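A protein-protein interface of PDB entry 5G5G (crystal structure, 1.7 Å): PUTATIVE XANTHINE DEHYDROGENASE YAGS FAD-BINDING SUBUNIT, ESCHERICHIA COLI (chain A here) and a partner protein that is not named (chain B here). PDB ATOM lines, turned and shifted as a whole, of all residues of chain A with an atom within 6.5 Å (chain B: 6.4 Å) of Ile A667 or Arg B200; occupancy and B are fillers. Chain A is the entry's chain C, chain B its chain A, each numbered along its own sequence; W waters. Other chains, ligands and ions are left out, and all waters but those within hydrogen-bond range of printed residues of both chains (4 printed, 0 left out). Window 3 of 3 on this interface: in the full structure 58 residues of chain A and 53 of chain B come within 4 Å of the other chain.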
ATOM      1  N   VAL A 604      16.974   2.675  20.364  1.00  0.00           N
ATOM      2  CA  VAL A 604      16.479   1.406  19.883  1.00  0.00           C
ATOM      3  C   VAL A 604      15.779   0.652  20.990  1.00  0.00           C
ATOM      4  O   VAL A 604      16.318   0.503  22.082  1.00  0.00           O
ATOM      5  CB  VAL A 604      17.593   0.563  19.282  1.00  0.00           C
ATOM      6  CG1 VAL A 604      17.048  -0.719  18.613  1.00  0.00           C
ATOM      7  CG2 VAL A 604      18.354   1.401  18.258  1.00  0.00           C
ATOM      8  N   THR A 631      24.912  -4.496  17.472  1.00  0.00           N
ATOM      9  CA  THR A 631      25.412  -3.339  18.167  1.00  0.00           C
ATOM     10  C   THR A 631      26.265  -2.437  17.293  1.00  0.00           C
ATOM     11  O   THR A 631      26.064  -1.212  17.273  1.00  0.00           O
ATOM     12  CB  THR A 631      26.172  -3.835  19.423  1.00  0.00           C
ATOM     13  OG1 THR A 631      25.247  -4.635  20.206  1.00  0.00           O
ATOM     14  CG2 THR A 631      26.688  -2.643  20.186  1.00  0.00           C
ATOM     15  N   MET A 634      23.976  -0.615  15.027  1.00  0.00           N
ATOM     16  CA  MET A 634      23.353   0.505  15.753  1.00  0.00           C
ATOM     17  C   MET A 634      24.300   1.708  15.714  1.00  0.00           C
ATOM     18  O   MET A 634      23.853   2.853  15.508  1.00  0.00           O
ATOM     19  CB  MET A 634      23.004   0.148  17.190  1.00  0.00           C
ATOM     20  CG  MET A 634      22.009   1.118  17.818  1.00  0.00           C
ATOM     21  SD  MET A 634      21.842   0.997  19.595  1.00  0.00           S
ATOM     22  CE  MET A 634      21.336  -0.700  19.773  1.00  0.00           C
ATOM     23  N   PRO A 662      28.398   2.512  20.558  1.00  0.00           N
ATOM     24  CA  PRO A 662      27.318   2.298  21.501  1.00  0.00           C
ATOM     25  C   PRO A 662      27.820   1.885  22.887  1.00  0.00           C
ATOM     26  O   PRO A 662      28.829   1.228  22.979  1.00  0.00           O
ATOM     27  CB  PRO A 662      26.576   1.123  20.893  1.00  0.00           C
ATOM     28  CG  PRO A 662      26.761   1.334  19.418  1.00  0.00           C
ATOM     29  CD  PRO A 662      28.202   1.706  19.347  1.00  0.00           C
ATOM     30  N   VAL A 663      27.098   2.335  23.897  1.00  0.00           N
ATOM     31  CA  VAL A 663      27.392   2.043  25.284  1.00  0.00           C
ATOM     32  C   VAL A 663      26.261   1.173  25.864  1.00  0.00           C
ATOM     33  O   VAL A 663      25.179   0.999  25.236  1.00  0.00           O
ATOM     34  CB  VAL A 663      27.555   3.329  26.139  1.00  0.00           C
ATOM     35  CG1 VAL A 663      28.767   4.139  25.665  1.00  0.00           C
ATOM     36  CG2 VAL A 663      26.271   4.165  26.123  1.00  0.00           C
ATOM     37  N   HIS A 664      26.489   0.652  27.066  1.00  0.00           N
ATOM     38  CA  HIS A 664      25.478  -0.222  27.693  1.00  0.00           C
ATOM     39  C   HIS A 664      24.060   0.313  27.620  1.00  0.00           C
ATOM     40  O   HIS A 664      23.138  -0.419  27.205  1.00  0.00           O
ATOM     41  CB  HIS A 664      25.780  -0.508  29.137  1.00  0.00           C
ATOM     42  CG  HIS A 664      26.679  -1.664  29.386  1.00  0.00           C
ATOM     43  ND1 HIS A 664      26.186  -2.943  29.538  1.00  0.00           N
ATOM     44  CD2 HIS A 664      28.015  -1.733  29.675  1.00  0.00           C
ATOM     45  CE1 HIS A 664      27.176  -3.750  29.887  1.00  0.00           C
ATOM     46  NE2 HIS A 664      28.298  -3.038  29.995  1.00  0.00           N
ATOM     47  N   ALA A 665      23.892   1.592  27.961  1.00  0.00           N
ATOM     48  CA  ALA A 665      22.601   2.240  28.004  1.00  0.00           C
ATOM     49  C   ALA A 665      21.861   2.296  26.641  1.00  0.00           C
ATOM     50  O   ALA A 665      20.657   2.491  26.616  1.00  0.00           O
ATOM     51  CB  ALA A 665      22.721   3.613  28.609  1.00  0.00           C
ATOM     52  N   ASP A 666      22.585   2.203  25.546  1.00  0.00           N
ATOM     53  CA  ASP A 666      22.016   2.186  24.203  1.00  0.00           C
ATOM     54  C   ASP A 666      21.351   0.838  23.820  1.00  0.00           C
ATOM     55  O   ASP A 666      20.621   0.796  22.837  1.00  0.00           O
ATOM     56  CB  ASP A 666      23.130   2.421  23.161  1.00  0.00           C
ATOM     57  CG  ASP A 666      23.679   3.827  23.189  1.00  0.00           C
ATOM     58  OD1 ASP A 666      22.848   4.782  23.226  1.00  0.00           O
ATOM     59  OD2 ASP A 666      24.946   3.978  23.195  1.00  0.00           O
ATOM     60  N   ILE A 667      21.617  -0.239  24.561  1.00  0.00           N
ATOM     61  CA  ILE A 667      21.380  -1.567  24.043  1.00  0.00           C
ATOM     62  C   ILE A 667      20.020  -2.062  24.451  1.00  0.00           C
ATOM     63  O   ILE A 667      19.743  -2.129  25.624  1.00  0.00           O
ATOM     64  CB  ILE A 667      22.438  -2.593  24.529  1.00  0.00           C
ATOM     65  CG1 ILE A 667      23.851  -2.049  24.305  1.00  0.00           C
ATOM     66  CG2 ILE A 667      22.233  -3.940  23.789  1.00  0.00           C
ATOM     67  CD1 ILE A 667      24.133  -1.638  22.877  1.00  0.00           C
ATOM     68  N   PRO A 668      19.181  -2.452  23.474  1.00  0.00           N
ATOM     69  CA  PRO A 668      17.854  -2.983  23.703  1.00  0.00           C
ATOM     70  C   PRO A 668      17.930  -4.481  23.861  1.00  0.00           C
ATOM     71  O   PRO A 668      19.031  -5.102  23.843  1.00  0.00           O
ATOM     72  CB  PRO A 668      17.134  -2.654  22.420  1.00  0.00           C
ATOM     73  CG  PRO A 668      18.169  -2.837  21.401  1.00  0.00           C
ATOM     74  CD  PRO A 668      19.477  -2.395  22.041  1.00  0.00           C
ATOM     75  N   LYS A 669      16.732  -5.049  24.017  1.00  0.00           N
ATOM     76  CA  LYS A 669      16.569  -6.471  23.856  1.00  0.00           C
ATOM     77  C   LYS A 669      17.082  -6.826  22.459  1.00  0.00           C
ATOM     78  O   LYS A 669      16.672  -6.196  21.486  1.00  0.00           O
ATOM     79  CB  LYS A 669      15.086  -6.787  24.011  1.00  0.00           C
ATOM     80  CG  LYS A 669      14.620  -8.196  23.733  1.00  0.00           C
ATOM     81  CD  LYS A 669      13.085  -8.191  23.903  1.00  0.00           C
ATOM     82  CE  LYS A 669      12.349  -8.736  22.715  1.00  0.00           C
ATOM     83  NZ  LYS A 669      12.559 -10.203  22.770  1.00  0.00           N
ATOM     84  N   GLN A 670      17.978  -7.806  22.386  1.00  0.00           N
ATOM     85  CA  GLN A 670      18.521  -8.315  21.095  1.00  0.00           C
ATOM     86  C   GLN A 670      18.308  -9.838  20.979  1.00  0.00           C
ATOM     87  O   GLN A 670      18.869 -10.615  21.768  1.00  0.00           O
ATOM     88  CB  GLN A 670      19.982  -7.987  20.960  1.00  0.00           C
ATOM     89  CG  GLN A 670      20.266  -6.500  20.893  1.00  0.00           C
ATOM     90  CD  GLN A 670      21.770  -6.185  20.922  1.00  0.00           C
ATOM     91  OE1 GLN A 670      22.577  -6.845  21.619  1.00  0.00           O
ATOM     92  NE2 GLN A 670      22.141  -5.167  20.195  1.00  0.00           N
ATOM     93  N   THR B 195      17.504  -3.137  38.730  1.00  0.00           N
ATOM     94  CA  THR B 195      16.738  -3.426  37.538  1.00  0.00           C
ATOM     95  C   THR B 195      17.691  -3.426  36.370  1.00  0.00           C
ATOM     96  O   THR B 195      18.768  -2.853  36.467  1.00  0.00           O
ATOM     97  CB  THR B 195      15.673  -2.351  37.308  1.00  0.00           C
ATOM     98  OG1 THR B 195      16.310  -1.110  36.972  1.00  0.00           O
ATOM     99  CG2 THR B 195      14.793  -2.175  38.536  1.00  0.00           C
ATOM    100  N   ALA B 196      17.282  -4.007  35.244  1.00  0.00           N
ATOM    101  CA  ALA B 196      18.053  -3.971  34.001  1.00  0.00           C
ATOM    102  C   ALA B 196      18.452  -2.539  33.594  1.00  0.00           C
ATOM    103  O   ALA B 196      19.587  -2.282  33.223  1.00  0.00           O
ATOM    104  CB  ALA B 196      17.221  -4.590  32.875  1.00  0.00           C
ATOM    105  N   ASP B 197      17.494  -1.624  33.697  1.00  0.00           N
ATOM    106  CA  ASP B 197      17.720  -0.236  33.302  1.00  0.00           C
ATOM    107  C   ASP B 197      18.805   0.408  34.146  1.00  0.00           C
ATOM    108  O   ASP B 197      19.686   1.079  33.615  1.00  0.00           O
ATOM    109  CB  ASP B 197      16.433   0.595  33.396  1.00  0.00           C
ATOM    110  CG  ASP B 197      16.505   1.873  32.573  1.00  0.00           C
ATOM    111  OD1 ASP B 197      17.189   1.867  31.510  1.00  0.00           O
ATOM    112  OD2 ASP B 197      15.895   2.891  32.980  1.00  0.00           O
ATOM    113  N   GLU B 198      18.710   0.212  35.458  1.00  0.00           N
ATOM    114  CA  GLU B 198      19.728   0.689  36.422  1.00  0.00           C
ATOM    115  C   GLU B 198      21.105   0.113  36.098  1.00  0.00           C
ATOM    116  O   GLU B 198      22.096   0.830  36.057  1.00  0.00           O
ATOM    117  CB  GLU B 198      19.327   0.375  37.859  1.00  0.00           C
ATOM    118  CG  GLU B 198      18.205   1.258  38.379  1.00  0.00           C
ATOM    119  CD  GLU B 198      18.631   2.645  38.830  1.00  0.00           C
ATOM    120  OE1 GLU B 198      19.826   2.994  38.704  1.00  0.00           O
ATOM    121  OE2 GLU B 198      17.732   3.367  39.358  1.00  0.00           O
ATOM    122  N   ILE B 199      21.157  -1.193  35.841  1.00  0.00           N
ATOM    123  CA  ILE B 199      22.443  -1.813  35.557  1.00  0.00           C
ATOM    124  C   ILE B 199      23.043  -1.270  34.259  1.00  0.00           C
ATOM    125  O   ILE B 199      24.259  -1.002  34.195  1.00  0.00           O
ATOM    126  CB  ILE B 199      22.344  -3.367  35.493  1.00  0.00           C
ATOM    127  CG1 ILE B 199      21.973  -3.920  36.864  1.00  0.00           C
ATOM    128  CG2 ILE B 199      23.662  -3.952  35.001  1.00  0.00           C
ATOM    129  CD1 ILE B 199      21.308  -5.284  36.770  1.00  0.00           C
ATOM    130  N   ARG B 200      22.227  -1.110  33.215  1.00  0.00           N
ATOM    131  CA  ARG B 200      22.760  -0.638  31.933  1.00  0.00           C
ATOM    132  C   ARG B 200      23.361   0.768  32.104  1.00  0.00           C
ATOM    133  O   ARG B 200      24.434   1.077  31.599  1.00  0.00           O
ATOM    134  CB  ARG B 200      21.653  -0.550  30.884  1.00  0.00           C
ATOM    135  CG  ARG B 200      21.218  -1.862  30.287  1.00  0.00           C
ATOM    136  CD  ARG B 200      20.332  -1.612  29.082  1.00  0.00           C
ATOM    137  NE  ARG B 200      19.769  -2.824  28.470  1.00  0.00           N
ATOM    138  CZ  ARG B 200      18.631  -3.392  28.827  1.00  0.00           C
ATOM    139  NH1 ARG B 200      17.947  -2.920  29.857  1.00  0.00           N
ATOM    140  NH2 ARG B 200      18.184  -4.447  28.159  1.00  0.00           N
ATOM    141  N   GLU B 201      22.659   1.613  32.841  1.00  0.00           N
ATOM    142  CA  GLU B 201      23.137   2.977  33.023  1.00  0.00           C
ATOM    143  C   GLU B 201      24.427   2.983  33.833  1.00  0.00           C
ATOM    144  O   GLU B 201      25.412   3.656  33.475  1.00  0.00           O
ATOM    145  CB  GLU B 201      22.082   3.863  33.666  1.00  0.00           C
ATOM    146  CG  GLU B 201      22.652   5.170  34.236  1.00  0.00           C
ATOM    147  CD  GLU B 201      23.316   6.092  33.222  1.00  0.00           C
ATOM    148  OE1 GLU B 201      23.024   5.995  32.008  1.00  0.00           O
ATOM    149  OE2 GLU B 201      24.135   6.935  33.647  1.00  0.00           O
ATOM    150  N   ARG B 202      24.433   2.202  34.897  1.00  0.00           N
ATOM    151  CA  ARG B 202      25.573   2.247  35.788  1.00  0.00           C
ATOM    152  C   ARG B 202      26.830   1.581  35.208  1.00  0.00           C
ATOM    153  O   ARG B 202      27.959   1.887  35.656  1.00  0.00           O
ATOM    154  CB  ARG B 202      25.205   1.656  37.141  1.00  0.00           C
ATOM    155  CG  ARG B 202      24.119   2.416  37.876  1.00  0.00           C
ATOM    156  CD  ARG B 202      23.503   1.531  38.934  1.00  0.00           C
ATOM    157  NE  ARG B 202      22.374   2.174  39.597  1.00  0.00           N
ATOM    158  CZ  ARG B 202      22.415   2.826  40.752  1.00  0.00           C
ATOM    159  NH1 ARG B 202      23.556   2.951  41.466  1.00  0.00           N
ATOM    160  NH2 ARG B 202      21.298   3.351  41.214  1.00  0.00           N
ATOM    161  N   MET B 203      26.654   0.699  34.234  1.00  0.00           N
ATOM    162  CA  MET B 203      27.766   0.072  33.513  1.00  0.00           C
ATOM    163  C   MET B 203      28.215   0.815  32.257  1.00  0.00           C
ATOM    164  O   MET B 203      29.084   0.302  31.533  1.00  0.00           O
ATOM    165  CB  MET B 203      27.381  -1.347  33.121  1.00  0.00           C
ATOM    166  CG  MET B 203      27.136  -2.284  34.280  1.00  0.00           C
ATOM    167  SD  MET B 203      28.702  -2.676  35.117  1.00  0.00           S
ATOM    168  CE  MET B 203      29.675  -3.386  33.792  1.00  0.00           C
ATOM    169  N   SER B 204      27.613   1.965  31.934  1.00  0.00           N
ATOM    170  CA  SER B 204      27.847   2.592  30.629  1.00  0.00           C
ATOM    171  C   SER B 204      29.258   3.180  30.477  1.00  0.00           C
ATOM    172  O   SER B 204      29.714   3.427  29.365  1.00  0.00           O
ATOM    173  CB  SER B 204      26.778   3.608  30.254  1.00  0.00           C
ATOM    174  OG  SER B 204      25.548   2.988  29.917  1.00  0.00           O
ATOM    175  N   GLY B 205      29.977   3.309  31.572  1.00  0.00           N
ATOM    176  CA  GLY B 205      31.374   3.635  31.524  1.00  0.00           C
ATOM    177  C   GLY B 205      32.316   2.505  31.203  1.00  0.00           C
ATOM    178  O   GLY B 205      33.517   2.714  31.326  1.00  0.00           O
ATOM    179  N   TYR B 213      27.285  -6.610  25.252  1.00  0.00           N
ATOM    180  CA  TYR B 213      26.421  -5.981  26.260  1.00  0.00           C
ATOM    181  C   TYR B 213      25.213  -6.769  26.733  1.00  0.00           C
ATOM    182  O   TYR B 213      24.942  -6.844  27.938  1.00  0.00           O
ATOM    183  CB  TYR B 213      25.944  -4.640  25.717  1.00  0.00           C
ATOM    184  CG  TYR B 213      26.988  -3.577  25.464  1.00  0.00           C
ATOM    185  CD1 TYR B 213      27.844  -3.155  26.449  1.00  0.00           C
ATOM    186  CD2 TYR B 213      27.160  -3.019  24.216  1.00  0.00           C
ATOM    187  CE1 TYR B 213      28.703  -2.104  26.228  1.00  0.00           C
ATOM    188  CE2 TYR B 213      28.051  -2.007  23.981  1.00  0.00           C
ATOM    189  CZ  TYR B 213      28.851  -1.571  24.973  1.00  0.00           C
ATOM    190  OH  TYR B 213      29.740  -0.519  24.751  1.00  0.00           O
ATOM    191  N   ALA B 214      24.414  -7.318  25.809  1.00  0.00           N
ATOM    192  CA  ALA B 214      23.224  -8.008  26.225  1.00  0.00           C
ATOM    193  C   ALA B 214      23.539  -9.219  27.084  1.00  0.00           C
ATOM    194  O   ALA B 214      22.833  -9.524  28.040  1.00  0.00           O
ATOM    195  CB  ALA B 214      22.370  -8.378  25.021  1.00  0.00           C
ATOM    196  N   LEU B 217      24.769  -7.968  30.626  1.00  0.00           N
ATOM    197  CA  LEU B 217      23.593  -7.727  31.466  1.00  0.00           C
ATOM    198  C   LEU B 217      23.035  -9.052  32.021  1.00  0.00           C
ATOM    199  O   LEU B 217      22.692  -9.118  33.222  1.00  0.00           O
ATOM    200  CB  LEU B 217      22.481  -6.998  30.689  1.00  0.00           C
ATOM    201  CG  LEU B 217      21.134  -6.731  31.353  1.00  0.00           C
ATOM    202  CD1 LEU B 217      21.369  -5.785  32.536  1.00  0.00           C
ATOM    203  CD2 LEU B 217      20.055  -6.199  30.356  1.00  0.00           C
HETATM  204  O   HOH W   1      18.856   1.583  28.781  1.00  0.00           O
HETATM  205  O   HOH W   2      19.895  -6.098  26.208  1.00  0.00           O
HETATM  206  O   HOH W   3      24.795  -6.773  23.072  1.00  0.00           O
HETATM  207  O   HOH W   4      29.217   1.077  27.872  1.00  0.00           O
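Of the 14 printed residues of chain B, 5 touch a printed residue of chain A. Printed residues of chain B that touch a printed residue of chain A: Arg B200, Met B203, Ser B204, Tyr B213 and Ala B214. Hydrophobic or aromatic side chains of chain B within 4 Å of the printed part of chain A: Met B203, Tyr B213 and Ala B214. Hydrophobic or aromatic side chains of chain A within 4 Å of the printed part of chain B: Val A663, His A664, Ala A665 and Ile A667. Among the printed residues, 12 pairs touch across the chains. Among the printed residues, no Asp or Glu carboxylate lies within 4 Å of a Lys or Arg side-chain nitrogen of the other chain.
NE of Arg B200 is in hydrogen-bond range of O of Ile A667 (2.9 Å). The backbone NH (N) of Ala A665 lies within hydrogen-bond range of the side-chain hydroxyl (OG) of Ser B204. O of Pro A662 is in hydrogen-bond range of OH of Tyr B213, at 2.6 Å.
The backbone carbonyl oxygen (O) of Arg B200 is in hydrogen-bond range of the side-chain hydroxyl (OG) of Ser B204, 2.8 Å away. The side-chain amide nitrogen of Gln A670 lies within hydrogen-bond range of the side-chain hydroxyl of Thr A631 (3.2 Å). The backbone NH (N) of Val A663 lies within hydrogen-bond range of the side-chain carboxylate (OD2) of Asp A666 (2.8 Å).
Of the printed residues of chain B, Val A663 touches Ser B204 (3.9 Å) and Tyr B213 (3.5 Å). Of the printed residues of chain B, His A664 touches Arg B200 (3.2 Å), Met B203 (3.0 Å), Ser B204 (3.6 Å) and Tyr B213 (3.5 Å). Of the printed residues of chain B, Ala A665 touches Arg B200 and Ser B204. Printed residues of chain B within 4 Å of Ile A667: Arg B200 (2.9 Å) and Tyr B213 (3.4 Å). Ile B199 touches none of the printed residues of chain A. Of the printed residues of chain A, Arg B200 touches His A664, Ala A665 and Ile A667. Gly B205 touches none of the printed residues of chain A. Of the printed residues of chain A, Tyr B213 touches Pro A662, Val A663, His A664 and Ile A667. The nearest printed residue of chain A that does not touch Arg B200 is Pro A668 (4.3 Å). The nearest printed residue of chain B that does not touch His A664 is Leu B217 (4.9 Å).
Water W3 lies within hydrogen-bond range of the side-chain amide oxygen (OE1) of Gln A670 (2.7 Å), the backbone NH (N) of Ala B214 (2.8 Å) and the backbone NH (N) of Tyr B213 (3.3 Å). Water W2 bridges the backbone carbonyl oxygen (O) of Pro A668 (2.7 Å) and the guanidinium group (NH2) of Arg B200 (3.1 Å). Water W4 lies within hydrogen-bond range of O of Ser B204 (2.8 Å) and N of His A664 (2.9 Å). Water W1 lies within hydrogen-bond range of O of Ala A665 and OD1 of Asp B197.
Ser B204 touches Val A663 (O to CB, 3.9 Å). Val A663 touches Tyr B213 (CA to OH, 3.5 Å). O of Arg B200 touches CB of His A664, at 3.2 Å. His A664 touches Met B203. CB of His A664 touches OG of Ser B204, at 3.6 Å. His A664 touches Tyr B213. Arg B200 touches Ala A665. CD2 of Tyr B213 touches CG1 of Ile A667, at 3.4 Å. OE1 of Gln A670 touches CB of Ala B214, at 3.7 Å.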
